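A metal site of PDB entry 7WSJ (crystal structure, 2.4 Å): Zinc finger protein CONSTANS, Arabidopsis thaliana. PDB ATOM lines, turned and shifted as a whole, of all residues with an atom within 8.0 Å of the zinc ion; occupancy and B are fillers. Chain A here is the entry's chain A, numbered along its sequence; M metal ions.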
ATOM      1  N   PRO A  20      19.638 -25.827   5.278  1.00  0.00           N
ATOM      2  CA  PRO A  20      18.584 -26.698   5.804  1.00  0.00           C
ATOM      3  C   PRO A  20      17.496 -25.896   6.499  1.00  0.00           C
ATOM      4  O   PRO A  20      17.683 -24.754   6.927  1.00  0.00           O
ATOM      5  CB  PRO A  20      19.326 -27.599   6.792  1.00  0.00           C
ATOM      6  CG  PRO A  20      20.482 -26.773   7.239  1.00  0.00           C
ATOM      7  CD  PRO A  20      20.901 -25.986   6.027  1.00  0.00           C
ATOM      8  N   CYS A  21      16.322 -26.520   6.575  1.00  0.00           N
ATOM      9  CA  CYS A  21      15.212 -25.924   7.314  1.00  0.00           C
ATOM     10  C   CYS A  21      15.538 -25.893   8.801  1.00  0.00           C
ATOM     11  O   CYS A  21      16.093 -26.844   9.363  1.00  0.00           O
ATOM     12  CB  CYS A  21      13.927 -26.721   7.081  1.00  0.00           C
ATOM     13  SG  CYS A  21      12.565 -26.235   8.154  1.00  0.00           S
ATOM     14  N   ASP A  22      15.203 -24.772   9.457  1.00  0.00           N
ATOM     15  CA  ASP A  22      15.572 -24.590  10.849  1.00  0.00           C
ATOM     16  C   ASP A  22      14.742 -25.427  11.808  1.00  0.00           C
ATOM     17  O   ASP A  22      15.198 -25.699  12.925  1.00  0.00           O
ATOM     18  CB  ASP A  22      15.479 -23.116  11.247  1.00  0.00           C
ATOM     19  CG  ASP A  22      16.674 -22.310  10.801  1.00  0.00           C
ATOM     20  OD1 ASP A  22      17.776 -22.884  10.699  1.00  0.00           O
ATOM     21  OD2 ASP A  22      16.526 -21.092  10.566  1.00  0.00           O
ATOM     22  N   THR A  23      13.540 -25.848  11.408  1.00  0.00           N
ATOM     23  CA  THR A  23      12.623 -26.517  12.322  1.00  0.00           C
ATOM     24  C   THR A  23      12.474 -28.006  12.059  1.00  0.00           C
ATOM     25  O   THR A  23      11.803 -28.690  12.846  1.00  0.00           O
ATOM     26  CB  THR A  23      11.241 -25.859  12.246  1.00  0.00           C
ATOM     27  OG1 THR A  23      10.858 -25.703  10.886  1.00  0.00           O
ATOM     28  CG2 THR A  23      11.261 -24.497  12.915  1.00  0.00           C
ATOM     29  N   CYS A  24      13.063 -28.536  10.988  1.00  0.00           N
ATOM     30  CA  CYS A  24      13.104 -29.970  10.759  1.00  0.00           C
ATOM     31  C   CYS A  24      14.463 -30.345  10.184  1.00  0.00           C
ATOM     32  O   CYS A  24      15.214 -29.488   9.708  1.00  0.00           O
ATOM     33  CB  CYS A  24      11.980 -30.447   9.832  1.00  0.00           C
ATOM     34  SG  CYS A  24      12.233 -30.055   8.091  1.00  0.00           S
ATOM     35  N   ARG A  25      14.776 -31.630  10.239  1.00  0.00           N
ATOM     36  CA  ARG A  25      16.092 -32.121   9.854  1.00  0.00           C
ATOM     37  C   ARG A  25      16.147 -32.712   8.450  1.00  0.00           C
ATOM     38  O   ARG A  25      17.253 -32.895   7.928  1.00  0.00           O
ATOM     39  CB  ARG A  25      16.588 -33.173  10.858  1.00  0.00           C
ATOM     40  CG  ARG A  25      16.882 -32.616  12.243  1.00  0.00           C
ATOM     41  CD  ARG A  25      17.790 -33.562  13.022  1.00  0.00           C
ATOM     42  NE  ARG A  25      18.045 -33.097  14.381  1.00  0.00           N
ATOM     43  CZ  ARG A  25      17.410 -33.553  15.460  1.00  0.00           C
ATOM     44  NH1 ARG A  25      16.483 -34.497  15.335  1.00  0.00           N
ATOM     45  NH2 ARG A  25      17.701 -33.073  16.653  1.00  0.00           N
ATOM     46  N   SER A  26      15.010 -33.009   7.837  1.00  0.00           N
ATOM     47  CA  SER A  26      14.989 -33.780   6.596  1.00  0.00           C
ATOM     48  C   SER A  26      14.829 -32.938   5.339  1.00  0.00           C
ATOM     49  O   SER A  26      14.935 -33.480   4.243  1.00  0.00           O
ATOM     50  CB  SER A  26      13.874 -34.826   6.649  1.00  0.00           C
ATOM     51  OG  SER A  26      12.634 -34.251   7.014  1.00  0.00           O
ATOM     52  N   ASN A  27      14.585 -31.628   5.459  1.00  0.00           N
ATOM     53  CA  ASN A  27      14.273 -30.800   4.304  1.00  0.00           C
ATOM     54  C   ASN A  27      15.186 -29.588   4.233  1.00  0.00           C
ATOM     55  O   ASN A  27      15.700 -29.109   5.253  1.00  0.00           O
ATOM     56  CB  ASN A  27      12.810 -30.327   4.339  1.00  0.00           C
ATOM     57  CG  ASN A  27      11.836 -31.431   4.015  1.00  0.00           C
ATOM     58  OD1 ASN A  27      12.208 -32.439   3.406  1.00  0.00           O
ATOM     59  ND2 ASN A  27      10.586 -31.255   4.415  1.00  0.00           N
ATOM     60  N   ALA A  28      15.404 -29.115   3.010  1.00  0.00           N
ATOM     61  CA  ALA A  28      16.080 -27.858   2.788  1.00  0.00           C
ATOM     62  C   ALA A  28      15.065 -26.716   2.858  1.00  0.00           C
ATOM     63  O   ALA A  28      13.877 -26.909   2.582  1.00  0.00           O
ATOM     64  CB  ALA A  28      16.793 -27.846   1.438  1.00  0.00           C
ATOM     65  N   CYS A  29      15.545 -25.535   3.223  1.00  0.00           N
ATOM     66  CA  CYS A  29      14.659 -24.388   3.352  1.00  0.00           C
ATOM     67  C   CYS A  29      14.188 -23.913   1.985  1.00  0.00           C
ATOM     68  O   CYS A  29      14.877 -24.074   0.976  1.00  0.00           O
ATOM     69  CB  CYS A  29      15.358 -23.252   4.096  1.00  0.00           C
ATOM     70  SG  CYS A  29      16.611 -22.394   3.113  1.00  0.00           S
ATOM     71  N   THR A  30      12.991 -23.336   1.963  1.00  0.00           N
ATOM     72  CA  THR A  30      12.484 -22.657   0.786  1.00  0.00           C
ATOM     73  C   THR A  30      12.099 -21.213   1.030  1.00  0.00           C
ATOM     74  O   THR A  30      12.104 -20.415   0.083  1.00  0.00           O
ATOM     75  CB  THR A  30      11.254 -23.397   0.217  1.00  0.00           C
ATOM     76  OG1 THR A  30      10.265 -23.534   1.238  1.00  0.00           O
ATOM     77  CG2 THR A  30      11.648 -24.760  -0.301  1.00  0.00           C
ATOM     78  N   TYR A  39      14.766 -19.805   8.608  1.00  0.00           N
ATOM     79  CA  TYR A  39      14.615 -20.420   7.292  1.00  0.00           C
ATOM     80  C   TYR A  39      13.775 -21.680   7.440  1.00  0.00           C
ATOM     81  O   TYR A  39      14.032 -22.491   8.347  1.00  0.00           O
ATOM     82  CB  TYR A  39      15.974 -20.751   6.685  1.00  0.00           C
ATOM     83  CG  TYR A  39      16.822 -19.548   6.324  1.00  0.00           C
ATOM     84  CD1 TYR A  39      17.565 -18.892   7.298  1.00  0.00           C
ATOM     85  CD2 TYR A  39      16.882 -19.079   5.020  1.00  0.00           C
ATOM     86  CE1 TYR A  39      18.349 -17.797   6.971  1.00  0.00           C
ATOM     87  CE2 TYR A  39      17.659 -17.991   4.688  1.00  0.00           C
ATOM     88  CZ  TYR A  39      18.393 -17.346   5.670  1.00  0.00           C
ATOM     89  OH  TYR A  39      19.164 -16.256   5.346  1.00  0.00           O
ATOM     90  N   LEU A  40      12.780 -21.833   6.581  1.00  0.00           N
ATOM     91  CA  LEU A  40      11.812 -22.916   6.716  1.00  0.00           C
ATOM     92  C   LEU A  40      11.547 -23.568   5.357  1.00  0.00           C
ATOM     93  O   LEU A  40      11.560 -22.895   4.324  1.00  0.00           O
ATOM     94  CB  LEU A  40      10.476 -22.401   7.283  1.00  0.00           C
ATOM     95  CG  LEU A  40      10.504 -21.698   8.643  1.00  0.00           C
ATOM     96  CD1 LEU A  40       9.139 -21.107   8.960  1.00  0.00           C
ATOM     97  CD2 LEU A  40      10.940 -22.664   9.726  1.00  0.00           C
ATOM     98  N   CYS A  41      11.319 -24.882   5.384  1.00  0.00           N
ATOM     99  CA  CYS A  41      10.725 -25.544   4.246  1.00  0.00           C
ATOM    100  C   CYS A  41       9.220 -25.256   4.216  1.00  0.00           C
ATOM    101  O   CYS A  41       8.662 -24.673   5.150  1.00  0.00           O
ATOM    102  CB  CYS A  41      10.983 -27.056   4.310  1.00  0.00           C
ATOM    103  SG  CYS A  41      10.167 -27.895   5.699  1.00  0.00           S
ATOM    104  N   MET A  42       8.576 -25.651   3.121  1.00  0.00           N
ATOM    105  CA  MET A  42       7.166 -25.297   2.949  1.00  0.00           C
ATOM    106  C   MET A  42       6.283 -25.969   3.992  1.00  0.00           C
ATOM    107  O   MET A  42       5.382 -25.335   4.553  1.00  0.00           O
ATOM    108  CB  MET A  42       6.709 -25.676   1.536  1.00  0.00           C
ATOM    109  CG  MET A  42       5.712 -24.682   0.973  1.00  0.00           C
ATOM    110  SD  MET A  42       6.366 -23.002   1.118  1.00  0.00           S
ATOM    111  CE  MET A  42       4.867 -22.037   0.963  1.00  0.00           C
ATOM    112  N   SER A  43       6.540 -27.244   4.280  1.00  0.00           N
ATOM    113  CA  SER A  43       5.798 -27.951   5.322  1.00  0.00           C
ATOM    114  C   SER A  43       5.897 -27.229   6.656  1.00  0.00           C
ATOM    115  O   SER A  43       4.883 -26.961   7.309  1.00  0.00           O
ATOM    116  CB  SER A  43       6.328 -29.385   5.440  1.00  0.00           C
ATOM    117  OG  SER A  43       5.880 -29.998   6.639  1.00  0.00           O
ATOM    118  N   CYS A  44       7.117 -26.899   7.073  1.00  0.00           N
ATOM    119  CA  CYS A  44       7.298 -26.218   8.350  1.00  0.00           C
ATOM    120  C   CYS A  44       6.771 -24.786   8.297  1.00  0.00           C
ATOM    121  O   CYS A  44       6.318 -24.267   9.322  1.00  0.00           O
ATOM    122  CB  CYS A  44       8.777 -26.228   8.730  1.00  0.00           C
ATOM    123  SG  CYS A  44       9.351 -27.818   9.353  1.00  0.00           S
ATOM    124  N   ASP A  45       6.831 -24.144   7.140  1.00  0.00           N
ATOM    125  CA  ASP A  45       6.225 -22.830   6.998  1.00  0.00           C
ATOM    126  C   ASP A  45       4.726 -22.890   7.299  1.00  0.00           C
ATOM    127  O   ASP A  45       4.205 -22.089   8.084  1.00  0.00           O
ATOM    128  CB  ASP A  45       6.468 -22.294   5.592  1.00  0.00           C
ATOM    129  CG  ASP A  45       5.942 -20.904   5.409  1.00  0.00           C
ATOM    130  OD1 ASP A  45       6.355 -20.033   6.195  1.00  0.00           O
ATOM    131  OD2 ASP A  45       5.126 -20.678   4.494  1.00  0.00           O
ATOM    132  N   GLN A  47       3.205 -25.257   8.998  1.00  0.00           N
ATOM    133  CA  GLN A  47       3.005 -25.649  10.385  1.00  0.00           C
ATOM    134  C   GLN A  47       3.174 -24.473  11.340  1.00  0.00           C
ATOM    135  O   GLN A  47       2.440 -24.336  12.317  1.00  0.00           O
ATOM    136  CB  GLN A  47       3.968 -26.770  10.755  1.00  0.00           C
ATOM    137  CG  GLN A  47       3.686 -28.089  10.044  1.00  0.00           C
ATOM    138  CD  GLN A  47       2.347 -28.670  10.418  1.00  0.00           C
ATOM    139  OE1 GLN A  47       1.973 -28.696  11.584  1.00  0.00           O
ATOM    140  NE2 GLN A  47       1.611 -29.154   9.420  1.00  0.00           N
ATOM    141  N   VAL A  48       4.146 -23.600  11.054  1.00  0.00           N
ATOM    142  CA  VAL A  48       4.448 -22.500  11.958  1.00  0.00           C
ATOM    143  C   VAL A  48       3.410 -21.393  11.838  1.00  0.00           C
ATOM    144  O   VAL A  48       2.969 -20.826  12.851  1.00  0.00           O
ATOM    145  CB  VAL A  48       5.870 -21.977  11.682  1.00  0.00           C
ATOM    146  CG1 VAL A  48       6.066 -20.607  12.331  1.00  0.00           C
ATOM    147  CG2 VAL A  48       6.902 -22.956  12.194  1.00  0.00           C
HETATM  148 ZN    ZN M   1      11.106 -28.029   7.834  1.00  0.00          ZN
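Thr 23 touches the zinc ion.
Of the 20 residues printed, 5 come within 4 Å of the zinc ion.
The nearest printed residue that does not touch the zinc ion is Asn 27 (4.5 Å).
The side-chain sulfur of Cys 44 sits close to the side-chain hydroxyl of Thr 23 (3.0 Å).
The side-chain hydroxyl of Thr 23 sits close to the side-chain sulfur of Cys 21 (3.3 Å).
N of Cys 21 sits at hydrogen-bond distance from O of Asn 27, at 3.0 Å.
The side-chain sulfur of Cys 41 sits close to the side-chain amide nitrogen of Asn 27.
The zinc ion is bound by SG of Cys 44, SG of Cys 24, SG of Cys 21 and SG of Cys 41.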
